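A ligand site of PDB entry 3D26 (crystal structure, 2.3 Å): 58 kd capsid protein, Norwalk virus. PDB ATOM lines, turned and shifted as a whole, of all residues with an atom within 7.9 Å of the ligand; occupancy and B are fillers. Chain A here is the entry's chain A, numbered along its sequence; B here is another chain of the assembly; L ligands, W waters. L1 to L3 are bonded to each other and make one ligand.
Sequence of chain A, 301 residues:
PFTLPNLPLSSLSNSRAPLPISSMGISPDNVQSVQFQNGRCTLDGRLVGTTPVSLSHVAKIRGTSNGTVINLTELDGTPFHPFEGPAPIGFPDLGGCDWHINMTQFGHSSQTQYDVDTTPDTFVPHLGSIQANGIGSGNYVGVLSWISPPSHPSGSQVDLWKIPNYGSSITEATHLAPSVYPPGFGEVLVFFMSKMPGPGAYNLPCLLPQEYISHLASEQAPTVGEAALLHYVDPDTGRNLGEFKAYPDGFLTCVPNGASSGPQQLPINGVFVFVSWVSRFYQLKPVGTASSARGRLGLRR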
ATOM      1  N   CYS A  97      22.815  15.796  -9.347  1.00  0.00           N
ATOM      2  CA  CYS A  97      22.354  14.419  -9.241  1.00  0.00           C
ATOM      3  C   CYS A  97      21.850  13.931 -10.591  1.00  0.00           C
ATOM      4  O   CYS A  97      21.584  14.737 -11.490  1.00  0.00           O
ATOM      5  CB  CYS A  97      21.209  14.285  -8.219  1.00  0.00           C
ATOM      6  SG  CYS A  97      19.618  15.107  -8.665  1.00  0.00           S
ATOM      7  N   ASP A  98      21.744  12.620 -10.736  1.00  0.00           N
ATOM      8  CA  ASP A  98      21.216  12.025 -11.954  1.00  0.00           C
ATOM      9  C   ASP A  98      19.751  11.693 -11.644  1.00  0.00           C
ATOM     10  O   ASP A  98      19.423  11.353 -10.501  1.00  0.00           O
ATOM     11  CB  ASP A  98      21.978  10.761 -12.305  1.00  0.00           C
ATOM     12  CG  ASP A  98      23.111  11.009 -13.269  1.00  0.00           C
ATOM     13  OD1 ASP A  98      23.570  12.158 -13.389  1.00  0.00           O
ATOM     14  OD2 ASP A  98      23.534  10.022 -13.899  1.00  0.00           O
ATOM     15  N   TRP A  99      18.878  11.809 -12.648  1.00  0.00           N
ATOM     16  CA  TRP A  99      17.468  11.516 -12.417  1.00  0.00           C
ATOM     17  C   TRP A  99      17.039  10.207 -13.026  1.00  0.00           C
ATOM     18  O   TRP A  99      17.600   9.736 -14.021  1.00  0.00           O
ATOM     19  CB  TRP A  99      16.556  12.592 -13.005  1.00  0.00           C
ATOM     20  CG  TRP A  99      16.870  13.981 -12.636  1.00  0.00           C
ATOM     21  CD1 TRP A  99      17.488  14.429 -11.506  1.00  0.00           C
ATOM     22  CD2 TRP A  99      16.522  15.136 -13.401  1.00  0.00           C
ATOM     23  NE1 TRP A  99      17.551  15.798 -11.527  1.00  0.00           N
ATOM     24  CE2 TRP A  99      16.975  16.257 -12.680  1.00  0.00           C
ATOM     25  CE3 TRP A  99      15.885  15.329 -14.630  1.00  0.00           C
ATOM     26  CZ2 TRP A  99      16.794  17.569 -13.151  1.00  0.00           C
ATOM     27  CZ3 TRP A  99      15.706  16.618 -15.103  1.00  0.00           C
ATOM     28  CH2 TRP A  99      16.158  17.720 -14.363  1.00  0.00           C
ATOM     29  N   HIS A 100      15.998   9.639 -12.441  1.00  0.00           N
ATOM     30  CA  HIS A 100      15.429   8.400 -12.921  1.00  0.00           C
ATOM     31  C   HIS A 100      13.930   8.644 -12.891  1.00  0.00           C
ATOM     32  O   HIS A 100      13.290   8.611 -11.833  1.00  0.00           O
ATOM     33  CB  HIS A 100      15.838   7.263 -12.002  1.00  0.00           C
ATOM     34  CG  HIS A 100      17.315   7.130 -11.876  1.00  0.00           C
ATOM     35  ND1 HIS A 100      18.114   6.704 -12.926  1.00  0.00           N
ATOM     36  CD2 HIS A 100      18.167   7.432 -10.867  1.00  0.00           C
ATOM     37  CE1 HIS A 100      19.373   6.741 -12.561  1.00  0.00           C
ATOM     38  NE2 HIS A 100      19.442   7.177 -11.317  1.00  0.00           N
ATOM     39  N   GLN A 113      12.018   3.001 -17.136  1.00  0.00           N
ATOM     40  CA  GLN A 113      12.857   3.867 -16.327  1.00  0.00           C
ATOM     41  C   GLN A 113      13.691   4.747 -17.261  1.00  0.00           C
ATOM     42  O   GLN A 113      14.336   4.250 -18.177  1.00  0.00           O
ATOM     43  CB  GLN A 113      13.772   3.061 -15.417  1.00  0.00           C
ATOM     44  CG  GLN A 113      14.420   3.900 -14.338  1.00  0.00           C
ATOM     45  CD  GLN A 113      15.409   3.108 -13.512  1.00  0.00           C
ATOM     46  OE1 GLN A 113      16.506   2.798 -13.966  1.00  0.00           O
ATOM     47  NE2 GLN A 113      15.017   2.772 -12.277  1.00  0.00           N
ATOM     48  N   ASP A 115      16.763   7.196 -17.443  1.00  0.00           N
ATOM     49  CA  ASP A 115      17.994   7.671 -16.819  1.00  0.00           C
ATOM     50  C   ASP A 115      18.366   9.003 -17.436  1.00  0.00           C
ATOM     51  O   ASP A 115      18.562   9.098 -18.645  1.00  0.00           O
ATOM     52  CB  ASP A 115      19.110   6.645 -17.048  1.00  0.00           C
ATOM     53  CG  ASP A 115      18.750   5.246 -16.550  1.00  0.00           C
ATOM     54  OD1 ASP A 115      19.517   4.299 -16.827  1.00  0.00           O
ATOM     55  OD2 ASP A 115      17.704   5.093 -15.881  1.00  0.00           O
ATOM     56  N   VAL A 116      18.479  10.026 -16.599  1.00  0.00           N
ATOM     57  CA  VAL A 116      18.817  11.359 -17.085  1.00  0.00           C
ATOM     58  C   VAL A 116      20.072  11.935 -16.466  1.00  0.00           C
ATOM     59  O   VAL A 116      20.190  12.020 -15.246  1.00  0.00           O
ATOM     60  CB  VAL A 116      17.664  12.362 -16.799  1.00  0.00           C
ATOM     61  CG1 VAL A 116      17.968  13.702 -17.442  1.00  0.00           C
ATOM     62  CG2 VAL A 116      16.352  11.816 -17.318  1.00  0.00           C
ATOM     63  N   ASP A 117      21.010  12.325 -17.322  1.00  0.00           N
ATOM     64  CA  ASP A 117      22.250  12.945 -16.903  1.00  0.00           C
ATOM     65  C   ASP A 117      22.095  14.383 -17.363  1.00  0.00           C
ATOM     66  O   ASP A 117      22.039  14.647 -18.563  1.00  0.00           O
ATOM     67  CB  ASP A 117      23.431  12.285 -17.596  1.00  0.00           C
ATOM     68  CG  ASP A 117      24.739  12.951 -17.258  1.00  0.00           C
ATOM     69  OD1 ASP A 117      25.783  12.522 -17.808  1.00  0.00           O
ATOM     70  OD2 ASP A 117      24.734  13.892 -16.431  1.00  0.00           O
ATOM     71  N   ASN A 133      17.564   8.592 -23.533  1.00  0.00           N
ATOM     72  CA  ASN A 133      18.618   7.649 -23.157  1.00  0.00           C
ATOM     73  C   ASN A 133      18.208   6.217 -23.402  1.00  0.00           C
ATOM     74  O   ASN A 133      18.336   5.361 -22.531  1.00  0.00           O
ATOM     75  CB  ASN A 133      18.989   7.839 -21.685  1.00  0.00           C
ATOM     76  CG  ASN A 133      20.255   7.114 -21.317  1.00  0.00           C
ATOM     77  OD1 ASN A 133      20.597   7.002 -20.140  1.00  0.00           O
ATOM     78  ND2 ASN A 133      20.974   6.609 -22.320  1.00  0.00           N
ATOM     79  N   TRP A 146      13.394   8.379  -8.452  1.00  0.00           N
ATOM     80  CA  TRP A 146      14.482   8.321  -7.480  1.00  0.00           C
ATOM     81  C   TRP A 146      15.699   8.982  -8.112  1.00  0.00           C
ATOM     82  O   TRP A 146      15.745   9.137  -9.328  1.00  0.00           O
ATOM     83  CB  TRP A 146      14.793   6.861  -7.096  1.00  0.00           C
ATOM     84  CG  TRP A 146      15.155   5.954  -8.248  1.00  0.00           C
ATOM     85  CD1 TRP A 146      14.302   5.374  -9.149  1.00  0.00           C
ATOM     86  CD2 TRP A 146      16.477   5.509  -8.619  1.00  0.00           C
ATOM     87  NE1 TRP A 146      15.005   4.604 -10.051  1.00  0.00           N
ATOM     88  CE2 TRP A 146      16.338   4.671  -9.744  1.00  0.00           C
ATOM     89  CE3 TRP A 146      17.762   5.750  -8.092  1.00  0.00           C
ATOM     90  CZ2 TRP A 146      17.435   4.068 -10.361  1.00  0.00           C
ATOM     91  CZ3 TRP A 146      18.864   5.149  -8.717  1.00  0.00           C
ATOM     92  CH2 TRP A 146      18.687   4.316  -9.829  1.00  0.00           C
ATOM     93  N   ILE A 147      16.665   9.382  -7.302  1.00  0.00           N
ATOM     94  CA  ILE A 147      17.864  10.025  -7.831  1.00  0.00           C
ATOM     95  C   ILE A 147      19.119   9.267  -7.417  1.00  0.00           C
ATOM     96  O   ILE A 147      19.040   8.291  -6.671  1.00  0.00           O
ATOM     97  CB  ILE A 147      17.993  11.506  -7.345  1.00  0.00           C
ATOM     98  CG1 ILE A 147      18.124  11.548  -5.823  1.00  0.00           C
ATOM     99  CG2 ILE A 147      16.782  12.314  -7.807  1.00  0.00           C
ATOM    100  CD1 ILE A 147      18.483  12.915  -5.280  1.00  0.00           C
ATOM    101  N   SER A 148      20.265   9.706  -7.926  1.00  0.00           N
ATOM    102  CA  SER A 148      21.553   9.085  -7.624  1.00  0.00           C
ATOM    103  C   SER A 148      22.664  10.115  -7.877  1.00  0.00           C
ATOM    104  O   SER A 148      22.398  11.196  -8.397  1.00  0.00           O
ATOM    105  CB  SER A 148      21.751   7.851  -8.501  1.00  0.00           C
ATOM    106  OG  SER A 148      21.551   8.201  -9.863  1.00  0.00           O
ATOM    107  N   PRO A 149      23.917   9.800  -7.512  1.00  0.00           N
ATOM    108  CA  PRO A 149      25.040  10.730  -7.716  1.00  0.00           C
ATOM    109  C   PRO A 149      25.233  11.139  -9.180  1.00  0.00           C
ATOM    110  O   PRO A 149      24.904  10.381 -10.089  1.00  0.00           O
ATOM    111  CB  PRO A 149      26.234   9.935  -7.179  1.00  0.00           C
ATOM    112  CG  PRO A 149      25.601   8.987  -6.164  1.00  0.00           C
ATOM    113  CD  PRO A 149      24.381   8.536  -6.907  1.00  0.00           C
ATOM    114  N   PRO A 150      25.788  12.341  -9.434  1.00  0.00           N
ATOM    115  CA  PRO A 150      26.000  12.782 -10.814  1.00  0.00           C
ATOM    116  C   PRO A 150      26.934  11.861 -11.607  1.00  0.00           C
ATOM    117  O   PRO A 150      27.975  11.437 -11.089  1.00  0.00           O
ATOM    118  CB  PRO A 150      26.577  14.185 -10.653  1.00  0.00           C
ATOM    119  CG  PRO A 150      26.021  14.645  -9.332  1.00  0.00           C
ATOM    120  CD  PRO A 150      26.175  13.404  -8.481  1.00  0.00           C
ATOM    121  N   SER A 151      26.579  11.551 -12.856  1.00  0.00           N
ATOM    122  CA  SER A 151      27.396  10.687 -13.707  1.00  0.00           C
ATOM    123  C   SER A 151      28.695  11.366 -14.174  1.00  0.00           C
ATOM    124  O   SER A 151      29.748  10.727 -14.228  1.00  0.00           O
ATOM    125  CB  SER A 151      26.627  10.226 -14.960  1.00  0.00           C
ATOM    126  OG  SER A 151      25.708   9.183 -14.681  1.00  0.00           O
ATOM    127  N   HIS A 152      28.657  12.656 -14.497  1.00  0.00           N
ATOM    128  CA  HIS A 152      29.883  13.251 -14.984  1.00  0.00           C
ATOM    129  C   HIS A 152      30.730  14.120 -14.089  1.00  0.00           C
ATOM    130  O   HIS A 152      31.928  14.248 -14.338  1.00  0.00           O
ATOM    131  CB  HIS A 152      29.678  13.857 -16.344  1.00  0.00           C
ATOM    132  CG  HIS A 152      29.576  12.810 -17.399  1.00  0.00           C
ATOM    133  ND1 HIS A 152      30.534  11.828 -17.549  1.00  0.00           N
ATOM    134  CD2 HIS A 152      28.601  12.519 -18.291  1.00  0.00           C
ATOM    135  CE1 HIS A 152      30.142  10.969 -18.474  1.00  0.00           C
ATOM    136  NE2 HIS A 152      28.973  11.369 -18.940  1.00  0.00           N
ATOM    137  N   GLY A 155      32.533  11.120  -9.721  1.00  0.00           N
ATOM    138  CA  GLY A 155      32.751  10.887  -8.308  1.00  0.00           C
ATOM    139  C   GLY A 155      32.075  11.877  -7.380  1.00  0.00           C
ATOM    140  O   GLY A 155      32.026  11.652  -6.176  1.00  0.00           O
ATOM    141  N   SER A 156      31.540  12.967  -7.925  1.00  0.00           N
ATOM    142  CA  SER A 156      30.854  13.983  -7.104  1.00  0.00           C
ATOM    143  C   SER A 156      29.682  13.373  -6.344  1.00  0.00           C
ATOM    144  O   SER A 156      29.177  12.307  -6.692  1.00  0.00           O
ATOM    145  CB  SER A 156      30.356  15.139  -7.966  1.00  0.00           C
ATOM    146  OG  SER A 156      31.435  15.865  -8.528  1.00  0.00           O
ATOM    147  N   VAL A 158      25.723  13.746  -4.365  1.00  0.00           N
ATOM    148  CA  VAL A 158      24.397  14.325  -4.592  1.00  0.00           C
ATOM    149  C   VAL A 158      24.340  15.656  -3.852  1.00  0.00           C
ATOM    150  O   VAL A 158      24.614  15.704  -2.654  1.00  0.00           O
ATOM    151  CB  VAL A 158      23.274  13.398  -4.028  1.00  0.00           C
ATOM    152  CG1 VAL A 158      21.965  14.177  -3.912  1.00  0.00           C
ATOM    153  CG2 VAL A 158      23.095  12.197  -4.930  1.00  0.00           C
ATOM    154  N   PRO A 199      19.950   5.415  -3.769  1.00  0.00           N
ATOM    155  CA  PRO A 199      21.082   4.776  -3.094  1.00  0.00           C
ATOM    156  C   PRO A 199      21.847   5.621  -2.074  1.00  0.00           C
ATOM    157  O   PRO A 199      23.069   5.548  -1.980  1.00  0.00           O
ATOM    158  CB  PRO A 199      21.974   4.337  -4.255  1.00  0.00           C
ATOM    159  CG  PRO A 199      21.743   5.440  -5.251  1.00  0.00           C
ATOM    160  CD  PRO A 199      20.235   5.592  -5.206  1.00  0.00           C
ATOM    161  N   TYR A 202      19.337  10.797   0.830  1.00  0.00           N
ATOM    162  CA  TYR A 202      19.082  12.065   0.147  1.00  0.00           C
ATOM    163  C   TYR A 202      17.970  12.917   0.746  1.00  0.00           C
ATOM    164  O   TYR A 202      16.857  12.458   0.981  1.00  0.00           O
ATOM    165  CB  TYR A 202      18.786  11.767  -1.322  1.00  0.00           C
ATOM    166  CG  TYR A 202      19.877  10.953  -1.986  1.00  0.00           C
ATOM    167  CD1 TYR A 202      19.574  10.017  -2.976  1.00  0.00           C
ATOM    168  CD2 TYR A 202      21.207  11.086  -1.590  1.00  0.00           C
ATOM    169  CE1 TYR A 202      20.572   9.226  -3.539  1.00  0.00           C
ATOM    170  CE2 TYR A 202      22.210  10.296  -2.161  1.00  0.00           C
ATOM    171  CZ  TYR A 202      21.887   9.365  -3.126  1.00  0.00           C
ATOM    172  OH  TYR A 202      22.881   8.545  -3.637  1.00  0.00           O
ATOM    173  N   SER B 109      18.898   1.759  -5.024  1.00  0.00           N
ATOM    174  CA  SER B 109      18.633   2.224  -6.370  1.00  0.00           C
ATOM    175  C   SER B 109      17.594   1.347  -7.028  1.00  0.00           C
ATOM    176  O   SER B 109      17.207   0.312  -6.490  1.00  0.00           O
ATOM    177  CB  SER B 109      19.910   2.191  -7.202  1.00  0.00           C
ATOM    178  OG  SER B 109      20.954   2.870  -6.537  1.00  0.00           O
HETATM  179  C1  LIG L   1      26.102   4.766 -15.586  1.00  0.00           C
HETATM  180  C2  LIG L   1      26.564   6.175 -15.966  1.00  0.00           C
HETATM  181  C3  LIG L   1      27.914   6.115 -16.680  1.00  0.00           C
HETATM  182  C4  LIG L   1      27.805   5.137 -17.867  1.00  0.00           C
HETATM  183  C5  LIG L   1      27.311   3.784 -17.370  1.00  0.00           C
HETATM  184  C6  LIG L   1      27.217   2.805 -18.538  1.00  0.00           C
HETATM  185  O1  LIG L   1      26.687   6.979 -14.785  1.00  0.00           O
HETATM  186  O2  LIG L   1      28.272   7.415 -17.147  1.00  0.00           O
HETATM  187  O3  LIG L   1      26.863   5.656 -18.802  1.00  0.00           O
HETATM  188  O4  LIG L   1      26.029   3.933 -16.755  1.00  0.00           O
HETATM  189  C1  LG2 L   2      27.813   2.379 -13.384  1.00  0.00           C
HETATM  190  C2  LG2 L   2      26.656   2.930 -14.204  1.00  0.00           C
HETATM  191  C3  LG2 L   2      25.399   3.056 -13.345  1.00  0.00           C
HETATM  192  C4  LG2 L   2      25.152   1.733 -12.621  1.00  0.00           C
HETATM  193  C5  LG2 L   2      26.404   1.238 -11.912  1.00  0.00           C
HETATM  194  C6  LG2 L   2      26.134  -0.146 -11.303  1.00  0.00           C
HETATM  195  O1  LG2 L   2      28.968   2.262 -14.218  1.00  0.00           O
HETATM  196  O2  LG2 L   2      27.072   4.225 -14.674  1.00  0.00           O
HETATM  197  O3  LG2 L   2      25.715   4.104 -12.412  1.00  0.00           O
HETATM  198  O4  LG2 L   2      24.706   0.744 -13.550  1.00  0.00           O
HETATM  199  O5  LG2 L   2      27.487   1.094 -12.838  1.00  0.00           O
HETATM  200  O6  LG2 L   2      27.335  -0.636 -10.704  1.00  0.00           O
HETATM  201  C1  LG3 L   3      24.748   4.299 -11.366  1.00  0.00           C
HETATM  202  C2  LG3 L   3      23.515   5.098 -11.808  1.00  0.00           C
HETATM  203  C3  LG3 L   3      23.916   6.432 -12.431  1.00  0.00           C
HETATM  204  C4  LG3 L   3      24.899   7.159 -11.515  1.00  0.00           C
HETATM  205  C5  LG3 L   3      26.030   6.201 -11.121  1.00  0.00           C
HETATM  206  C6  LG3 L   3      27.100   6.873 -10.267  1.00  0.00           C
HETATM  207  C7  LG3 L   3      21.813   3.417 -12.282  1.00  0.00           C
HETATM  208  C8  LG3 L   3      20.959   2.734 -13.351  1.00  0.00           C
HETATM  209  N1  LG3 L   3      22.657   4.343 -12.727  1.00  0.00           N
HETATM  210  O1  LG3 L   3      22.737   7.239 -12.598  1.00  0.00           O
HETATM  211  O2  LG3 L   3      24.215   7.582 -10.331  1.00  0.00           O
HETATM  212  O3  LG3 L   3      25.462   5.086 -10.419  1.00  0.00           O
HETATM  213  O4  LG3 L   3      28.138   5.929 -10.006  1.00  0.00           O
HETATM  214  O5  LG3 L   3      21.714   3.096 -11.099  1.00  0.00           O
HETATM  215  O   HOH W   1      22.125   5.140 -15.662  1.00  0.00           O
HETATM  216  O   HOH W   2      22.165   3.662  -8.791  1.00  0.00           O
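The side-chain hydroxyl (OG) of Ser 148 sits at hydrogen-bond distance from an oxygen (O2) of LG3 L3 (2.8 Å).
An oxygen (O2) of LG3 L3 sits at hydrogen-bond distance from the backbone carbonyl oxygen of Pro 149 (2.9 Å).
The side-chain hydroxyl (OG) of Ser 151 is in hydrogen-bond range of an oxygen (O1) of LIG L1 (2.4 Å).
The side-chain carboxylate (OD2) of Asp 98 lies within hydrogen-bond range of an oxygen (O1) of LG3 L3.
The side-chain hydroxyl of Ser 151 lies within hydrogen-bond range of the side-chain carboxylate of Asp 98 (2.5 Å).
The backbone NH (N) of His 100 is in hydrogen-bond range of the backbone carbonyl oxygen (O) of Trp 146, at 3.2 Å.
NE2 of His 100 sits at hydrogen-bond distance from OG of Ser 148 (2.8 Å).
A ring nitrogen (ND1) of His 100 lies within hydrogen-bond range of the side-chain carboxylate (OD2) of Asp 115, at 3.4 Å.
O of Ser 148 is in hydrogen-bond range of N of Asp 98, at 2.8 Å.
NE1 of Trp 146 sits close to NE2 of Gln 113.
Merely in contact with the ligand: His 100 and Trp 146.
Hydrophobic or aromatic side chains that line the ligand: His 100, Trp 146 and Pro 149.
Within 4 Å of the ligand: Asp 98, His 100, Trp 146, Ser 148, Pro 149 and Ser 151.
Along chain A the residues within 4 Å of the ligand span positions 98 to 151.
Water W2 bridges an oxygen (O5) of LG3 L3 (2.4 Å) and the side-chain hydroxyl of Ser 109 of chain B (2.7 Å).
Water W1 bridges the side-chain carboxylate of Asp 115 and a nitrogen (N1) of LG3 L3.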
